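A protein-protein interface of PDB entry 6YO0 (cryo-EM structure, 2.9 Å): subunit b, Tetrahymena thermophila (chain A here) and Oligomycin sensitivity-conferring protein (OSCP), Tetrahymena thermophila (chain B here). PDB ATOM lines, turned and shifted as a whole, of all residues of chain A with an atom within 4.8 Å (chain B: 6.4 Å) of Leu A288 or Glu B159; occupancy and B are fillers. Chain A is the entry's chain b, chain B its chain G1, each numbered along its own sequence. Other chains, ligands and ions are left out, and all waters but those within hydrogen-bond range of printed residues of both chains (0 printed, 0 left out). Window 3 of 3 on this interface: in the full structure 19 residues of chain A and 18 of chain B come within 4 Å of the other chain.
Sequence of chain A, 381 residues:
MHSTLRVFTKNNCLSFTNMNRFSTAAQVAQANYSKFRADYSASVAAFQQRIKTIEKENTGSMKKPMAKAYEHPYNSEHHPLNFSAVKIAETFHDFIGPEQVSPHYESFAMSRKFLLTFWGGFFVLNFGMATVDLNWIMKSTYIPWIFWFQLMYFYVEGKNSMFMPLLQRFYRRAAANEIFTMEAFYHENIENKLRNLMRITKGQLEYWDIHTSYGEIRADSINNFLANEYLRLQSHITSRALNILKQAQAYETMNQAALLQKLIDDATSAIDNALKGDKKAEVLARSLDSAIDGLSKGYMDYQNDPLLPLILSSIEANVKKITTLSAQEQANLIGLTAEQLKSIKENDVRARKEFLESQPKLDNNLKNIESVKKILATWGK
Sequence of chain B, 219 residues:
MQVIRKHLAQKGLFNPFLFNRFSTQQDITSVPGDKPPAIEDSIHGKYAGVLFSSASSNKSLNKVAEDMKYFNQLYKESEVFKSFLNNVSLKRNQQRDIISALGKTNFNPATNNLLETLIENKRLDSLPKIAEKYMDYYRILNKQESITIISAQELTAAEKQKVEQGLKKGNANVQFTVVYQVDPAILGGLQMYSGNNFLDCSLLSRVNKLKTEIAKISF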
ATOM      1  N   LEU A 284     -23.256 -18.137  23.282  1.00  0.00           N
ATOM      2  CA  LEU A 284     -22.716 -17.979  21.939  1.00  0.00           C
ATOM      3  C   LEU A 284     -21.628 -19.010  21.685  1.00  0.00           C
ATOM      4  O   LEU A 284     -21.527 -19.562  20.584  1.00  0.00           O
ATOM      5  CB  LEU A 284     -22.180 -16.563  21.749  1.00  0.00           C
ATOM      6  CG  LEU A 284     -23.232 -15.478  21.508  1.00  0.00           C
ATOM      7  CD1 LEU A 284     -24.190 -15.371  22.674  1.00  0.00           C
ATOM      8  CD2 LEU A 284     -22.570 -14.142  21.252  1.00  0.00           C
ATOM      9  N   ALA A 285     -20.811 -19.285  22.702  1.00  0.00           N
ATOM     10  CA  ALA A 285     -19.782 -20.306  22.572  1.00  0.00           C
ATOM     11  C   ALA A 285     -20.409 -21.673  22.349  1.00  0.00           C
ATOM     12  O   ALA A 285     -19.979 -22.436  21.477  1.00  0.00           O
ATOM     13  CB  ALA A 285     -18.899 -20.309  23.819  1.00  0.00           C
ATOM     14  N   ARG A 286     -21.439 -21.997  23.132  1.00  0.00           N
ATOM     15  CA  ARG A 286     -22.113 -23.279  22.973  1.00  0.00           C
ATOM     16  C   ARG A 286     -22.797 -23.365  21.618  1.00  0.00           C
ATOM     17  O   ARG A 286     -22.824 -24.428  20.987  1.00  0.00           O
ATOM     18  CB  ARG A 286     -23.133 -23.470  24.093  1.00  0.00           C
ATOM     19  CG  ARG A 286     -23.823 -24.828  24.095  1.00  0.00           C
ATOM     20  CD  ARG A 286     -22.824 -25.959  24.208  1.00  0.00           C
ATOM     21  NE  ARG A 286     -21.856 -25.687  25.264  1.00  0.00           N
ATOM     22  CZ  ARG A 286     -22.091 -25.888  26.556  1.00  0.00           C
ATOM     23  NH1 ARG A 286     -21.153 -25.612  27.450  1.00  0.00           N
ATOM     24  NH2 ARG A 286     -23.266 -26.355  26.960  1.00  0.00           N
ATOM     25  N   SER A 287     -23.354 -22.248  21.150  1.00  0.00           N
ATOM     26  CA  SER A 287     -23.980 -22.220  19.835  1.00  0.00           C
ATOM     27  C   SER A 287     -22.950 -22.449  18.739  1.00  0.00           C
ATOM     28  O   SER A 287     -23.208 -23.185  17.779  1.00  0.00           O
ATOM     29  CB  SER A 287     -24.702 -20.893  19.625  1.00  0.00           C
ATOM     30  OG  SER A 287     -25.664 -20.680  20.642  1.00  0.00           O
ATOM     31  N   LEU A 288     -21.776 -21.829  18.865  1.00  0.00           N
ATOM     32  CA  LEU A 288     -20.723 -22.057  17.885  1.00  0.00           C
ATOM     33  C   LEU A 288     -20.343 -23.528  17.833  1.00  0.00           C
ATOM     34  O   LEU A 288     -20.193 -24.100  16.749  1.00  0.00           O
ATOM     35  CB  LEU A 288     -19.499 -21.215  18.239  1.00  0.00           C
ATOM     36  CG  LEU A 288     -19.593 -19.705  18.037  1.00  0.00           C
ATOM     37  CD1 LEU A 288     -18.310 -19.030  18.472  1.00  0.00           C
ATOM     38  CD2 LEU A 288     -19.889 -19.385  16.596  1.00  0.00           C
ATOM     39  N   ASP A 289     -20.206 -24.167  18.994  1.00  0.00           N
ATOM     40  CA  ASP A 289     -19.856 -25.582  19.006  1.00  0.00           C
ATOM     41  C   ASP A 289     -20.958 -26.406  18.355  1.00  0.00           C
ATOM     42  O   ASP A 289     -20.692 -27.278  17.520  1.00  0.00           O
ATOM     43  CB  ASP A 289     -19.609 -26.046  20.440  1.00  0.00           C
ATOM     44  CG  ASP A 289     -19.107 -27.473  20.513  1.00  0.00           C
ATOM     45  OD1 ASP A 289     -18.833 -28.064  19.447  1.00  0.00           O
ATOM     46  OD2 ASP A 289     -18.986 -28.004  21.636  1.00  0.00           O
ATOM     47  N   SER A 290     -22.208 -26.137  18.730  1.00  0.00           N
ATOM     48  CA  SER A 290     -23.329 -26.855  18.140  1.00  0.00           C
ATOM     49  C   SER A 290     -23.481 -26.529  16.661  1.00  0.00           C
ATOM     50  O   SER A 290     -23.855 -27.401  15.869  1.00  0.00           O
ATOM     51  CB  SER A 290     -24.617 -26.523  18.890  1.00  0.00           C
ATOM     52  OG  SER A 290     -25.702 -27.293  18.406  1.00  0.00           O
ATOM     53  N   ALA A 291     -23.186 -25.288  16.272  1.00  0.00           N
ATOM     54  CA  ALA A 291     -23.278 -24.917  14.865  1.00  0.00           C
ATOM     55  C   ALA A 291     -22.222 -25.627  14.030  1.00  0.00           C
ATOM     56  O   ALA A 291     -22.527 -26.144  12.951  1.00  0.00           O
ATOM     57  CB  ALA A 291     -23.142 -23.404  14.719  1.00  0.00           C
ATOM     58  N   ILE A 292     -20.986 -25.697  14.525  1.00  0.00           N
ATOM     59  CA  ILE A 292     -19.955 -26.435  13.802  1.00  0.00           C
ATOM     60  C   ILE A 292     -20.370 -27.887  13.644  1.00  0.00           C
ATOM     61  O   ILE A 292     -20.150 -28.503  12.594  1.00  0.00           O
ATOM     62  CB  ILE A 292     -18.595 -26.303  14.509  1.00  0.00           C
ATOM     63  CG1 ILE A 292     -17.874 -25.030  14.056  1.00  0.00           C
ATOM     64  CG2 ILE A 292     -17.730 -27.521  14.238  1.00  0.00           C
ATOM     65  CD1 ILE A 292     -18.568 -23.743  14.402  1.00  0.00           C
ATOM     66  N   SER B 151     -22.456 -14.892  10.425  1.00  0.00           N
ATOM     67  CA  SER B 151     -22.477 -14.936  11.881  1.00  0.00           C
ATOM     68  C   SER B 151     -22.473 -13.520  12.438  1.00  0.00           C
ATOM     69  O   SER B 151     -21.839 -12.628  11.870  1.00  0.00           O
ATOM     70  CB  SER B 151     -21.283 -15.708  12.438  1.00  0.00           C
ATOM     71  OG  SER B 151     -21.094 -15.416  13.812  1.00  0.00           O
ATOM     72  N   GLN B 153     -21.274 -12.531  15.556  1.00  0.00           N
ATOM     73  CA  GLN B 153     -19.995 -12.262  16.189  1.00  0.00           C
ATOM     74  C   GLN B 153     -18.866 -12.375  15.175  1.00  0.00           C
ATOM     75  O   GLN B 153     -18.918 -13.179  14.240  1.00  0.00           O
ATOM     76  CB  GLN B 153     -19.760 -13.233  17.343  1.00  0.00           C
ATOM     77  CG  GLN B 153     -18.758 -12.749  18.373  1.00  0.00           C
ATOM     78  CD  GLN B 153     -19.280 -12.869  19.789  1.00  0.00           C
ATOM     79  OE1 GLN B 153     -20.407 -12.478  20.084  1.00  0.00           O
ATOM     80  NE2 GLN B 153     -18.462 -13.428  20.673  1.00  0.00           N
ATOM     81  N   GLU B 154     -17.835 -11.558  15.364  1.00  0.00           N
ATOM     82  CA  GLU B 154     -16.671 -11.656  14.500  1.00  0.00           C
ATOM     83  C   GLU B 154     -16.016 -13.016  14.695  1.00  0.00           C
ATOM     84  O   GLU B 154     -15.895 -13.514  15.816  1.00  0.00           O
ATOM     85  CB  GLU B 154     -15.676 -10.532  14.794  1.00  0.00           C
ATOM     86  CG  GLU B 154     -16.319  -9.178  15.035  1.00  0.00           C
ATOM     87  CD  GLU B 154     -15.614  -8.063  14.291  1.00  0.00           C
ATOM     88  OE1 GLU B 154     -14.701  -7.442  14.872  1.00  0.00           O
ATOM     89  OE2 GLU B 154     -15.973  -7.808  13.121  1.00  0.00           O
ATOM     90  N   LEU B 155     -15.593 -13.616  13.590  1.00  0.00           N
ATOM     91  CA  LEU B 155     -15.036 -14.962  13.595  1.00  0.00           C
ATOM     92  C   LEU B 155     -13.537 -14.886  13.847  1.00  0.00           C
ATOM     93  O   LEU B 155     -12.786 -14.350  13.025  1.00  0.00           O
ATOM     94  CB  LEU B 155     -15.339 -15.663  12.276  1.00  0.00           C
ATOM     95  CG  LEU B 155     -16.809 -16.049  12.117  1.00  0.00           C
ATOM     96  CD1 LEU B 155     -17.593 -14.885  11.535  1.00  0.00           C
ATOM     97  CD2 LEU B 155     -16.962 -17.294  11.258  1.00  0.00           C
ATOM     98  N   THR B 156     -13.107 -15.384  15.002  1.00  0.00           N
ATOM     99  CA  THR B 156     -11.685 -15.450  15.301  1.00  0.00           C
ATOM    100  C   THR B 156     -10.998 -16.472  14.401  1.00  0.00           C
ATOM    101  O   THR B 156     -11.572 -17.502  14.039  1.00  0.00           O
ATOM    102  CB  THR B 156     -11.470 -15.824  16.767  1.00  0.00           C
ATOM    103  OG1 THR B 156     -12.085 -14.842  17.610  1.00  0.00           O
ATOM    104  CG2 THR B 156      -9.989 -15.911  17.086  1.00  0.00           C
ATOM    105  N   ALA B 157      -9.748 -16.168  14.036  1.00  0.00           N
ATOM    106  CA  ALA B 157      -9.012 -17.031  13.117  1.00  0.00           C
ATOM    107  C   ALA B 157      -8.998 -18.475  13.597  1.00  0.00           C
ATOM    108  O   ALA B 157      -9.169 -19.405  12.801  1.00  0.00           O
ATOM    109  CB  ALA B 157      -7.586 -16.515  12.947  1.00  0.00           C
ATOM    110  N   ALA B 158      -8.802 -18.683  14.900  1.00  0.00           N
ATOM    111  CA  ALA B 158      -8.828 -20.039  15.434  1.00  0.00           C
ATOM    112  C   ALA B 158     -10.194 -20.670  15.228  1.00  0.00           C
ATOM    113  O   ALA B 158     -10.300 -21.845  14.856  1.00  0.00           O
ATOM    114  CB  ALA B 158      -8.460 -20.026  16.916  1.00  0.00           C
ATOM    115  N   GLU B 159     -11.255 -19.899  15.463  1.00  0.00           N
ATOM    116  CA  GLU B 159     -12.602 -20.406  15.236  1.00  0.00           C
ATOM    117  C   GLU B 159     -12.821 -20.725  13.765  1.00  0.00           C
ATOM    118  O   GLU B 159     -13.446 -21.737  13.425  1.00  0.00           O
ATOM    119  CB  GLU B 159     -13.629 -19.385  15.726  1.00  0.00           C
ATOM    120  CG  GLU B 159     -15.046 -19.928  15.909  1.00  0.00           C
ATOM    121  CD  GLU B 159     -15.159 -21.019  16.969  1.00  0.00           C
ATOM    122  OE1 GLU B 159     -14.137 -21.635  17.333  1.00  0.00           O
ATOM    123  OE2 GLU B 159     -16.289 -21.265  17.441  1.00  0.00           O
ATOM    124  N   LYS B 160     -12.306 -19.874  12.875  1.00  0.00           N
ATOM    125  CA  LYS B 160     -12.488 -20.104  11.448  1.00  0.00           C
ATOM    126  C   LYS B 160     -11.856 -21.420  11.022  1.00  0.00           C
ATOM    127  O   LYS B 160     -12.414 -22.148  10.193  1.00  0.00           O
ATOM    128  CB  LYS B 160     -11.890 -18.948  10.652  1.00  0.00           C
ATOM    129  CG  LYS B 160     -12.810 -17.758  10.536  1.00  0.00           C
ATOM    130  CD  LYS B 160     -12.162 -16.613   9.780  1.00  0.00           C
ATOM    131  CE  LYS B 160     -11.380 -15.695  10.688  1.00  0.00           C
ATOM    132  NZ  LYS B 160     -11.361 -14.302  10.176  1.00  0.00           N
ATOM    133  N   GLN B 161     -10.690 -21.745  11.581  1.00  0.00           N
ATOM    134  CA  GLN B 161     -10.045 -23.008  11.243  1.00  0.00           C
ATOM    135  C   GLN B 161     -10.924 -24.182  11.645  1.00  0.00           C
ATOM    136  O   GLN B 161     -11.039 -25.166  10.905  1.00  0.00           O
ATOM    137  CB  GLN B 161      -8.677 -23.089  11.925  1.00  0.00           C
ATOM    138  CG  GLN B 161      -8.187 -24.500  12.254  1.00  0.00           C
ATOM    139  CD  GLN B 161      -8.192 -25.433  11.058  1.00  0.00           C
ATOM    140  OE1 GLN B 161      -8.576 -25.049   9.953  1.00  0.00           O
ATOM    141  NE2 GLN B 161      -7.772 -26.673  11.277  1.00  0.00           N
ATOM    142  N   LYS B 162     -11.567 -24.093  12.812  1.00  0.00           N
ATOM    143  CA  LYS B 162     -12.476 -25.152  13.226  1.00  0.00           C
ATOM    144  C   LYS B 162     -13.639 -25.266  12.255  1.00  0.00           C
ATOM    145  O   LYS B 162     -14.074 -26.372  11.915  1.00  0.00           O
ATOM    146  CB  LYS B 162     -12.984 -24.882  14.639  1.00  0.00           C
ATOM    147  CG  LYS B 162     -11.896 -24.877  15.687  1.00  0.00           C
ATOM    148  CD  LYS B 162     -12.467 -24.623  17.065  1.00  0.00           C
ATOM    149  CE  LYS B 162     -11.381 -24.660  18.128  1.00  0.00           C
ATOM    150  NZ  LYS B 162     -10.692 -25.978  18.180  1.00  0.00           N
ATOM    151  N   VAL B 163     -14.152 -24.125  11.795  1.00  0.00           N
ATOM    152  CA  VAL B 163     -15.258 -24.138  10.847  1.00  0.00           C
ATOM    153  C   VAL B 163     -14.845 -24.862   9.576  1.00  0.00           C
ATOM    154  O   VAL B 163     -15.615 -25.646   9.010  1.00  0.00           O
ATOM    155  CB  VAL B 163     -15.723 -22.699  10.560  1.00  0.00           C
ATOM    156  CG1 VAL B 163     -16.214 -22.561   9.133  1.00  0.00           C
ATOM    157  CG2 VAL B 163     -16.802 -22.294  11.536  1.00  0.00           C
ATOM    158  N   GLU B 164     -13.617 -24.626   9.117  1.00  0.00           N
ATOM    159  CA  GLU B 164     -13.143 -25.308   7.920  1.00  0.00           C
ATOM    160  C   GLU B 164     -13.111 -26.811   8.147  1.00  0.00           C
ATOM    161  O   GLU B 164     -13.467 -27.592   7.257  1.00  0.00           O
ATOM    162  CB  GLU B 164     -11.753 -24.801   7.541  1.00  0.00           C
ATOM    163  CG  GLU B 164     -11.615 -23.286   7.352  1.00  0.00           C
ATOM    164  CD  GLU B 164     -12.886 -22.588   6.906  1.00  0.00           C
ATOM    165  OE1 GLU B 164     -13.695 -23.194   6.176  1.00  0.00           O
ATOM    166  OE2 GLU B 164     -13.076 -21.417   7.293  1.00  0.00           O
ATOM    167  N   GLY B 188     -24.792 -15.470  17.675  1.00  0.00           N
ATOM    168  CA  GLY B 188     -24.143 -16.740  17.939  1.00  0.00           C
ATOM    169  C   GLY B 188     -24.503 -17.844  16.970  1.00  0.00           C
ATOM    170  O   GLY B 188     -24.214 -19.016  17.223  1.00  0.00           O
ATOM    171  N   GLY B 189     -25.134 -17.486  15.858  1.00  0.00           N
ATOM    172  CA  GLY B 189     -25.606 -18.449  14.884  1.00  0.00           C
ATOM    173  C   GLY B 189     -24.786 -18.442  13.610  1.00  0.00           C
ATOM    174  O   GLY B 189     -24.206 -17.421  13.233  1.00  0.00           O
ATOM    175  N   LEU B 190     -24.736 -19.596  12.949  1.00  0.00           N
ATOM    176  CA  LEU B 190     -24.041 -19.753  11.681  1.00  0.00           C
ATOM    177  C   LEU B 190     -25.039 -20.154  10.606  1.00  0.00           C
ATOM    178  O   LEU B 190     -25.851 -21.060  10.814  1.00  0.00           O
ATOM    179  CB  LEU B 190     -22.945 -20.814  11.775  1.00  0.00           C
ATOM    180  CG  LEU B 190     -21.662 -20.447  12.514  1.00  0.00           C
ATOM    181  CD1 LEU B 190     -20.903 -19.340  11.809  1.00  0.00           C
ATOM    182  CD2 LEU B 190     -21.983 -20.062  13.935  1.00  0.00           C
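Of chain B, only Glu B159 and Leu B190 come within 4 Å of Leu A288.
Of chain A, only Leu A288 comes within 4 Å of Glu B159.
Of the printed residues of chain A, Val B163 touches Ile A292 (3.7 Å).
Of the printed residues of chain A, Gly B188 touches Leu A284 (3.9 Å) and Ser A287 (3.1 Å).
The nearest residue of chain B that does not touch Leu A288 is Gly B188 (4.1 Å).
Hydrophobic or aromatic side chains of chain B within 4 Å of the printed part of chain A: Val B163 and Leu B190.
Along chain B the printed residues that touch a printed residue of chain A span positions 153 to 190.
Of the 9 printed residues of chain A, 5 touch a printed residue of chain B.
Printed residues of chain A that touch a printed residue of chain B: Leu A284, Ser A287, Leu A288, Ala A291 and Ile A292.
Hydrophobic or aromatic side chains of chain A within 4 Å of the printed part of chain B: Leu A284, Leu A288, Ala A291 and Ile A292.
The side-chain hydroxyl (OG) of Ser B151 sits at hydrogen-bond distance from the backbone carbonyl oxygen (O) of Gln B153 (3.1 Å).
Among the printed residues, pairs that only touch across the chains: Leu A284 with Gln B153 (3.0 Å), Ser A287 with Gly B188 (3.1 Å), Leu A288 with Glu B159 (3.2 Å), Leu A288 with Leu B190 (3.5 Å), Ala A291 with Leu B190 (3.6 Å), Ile A292 with Val B163 (3.7 Å) and Leu A284 with Gly B188 (3.9 Å).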
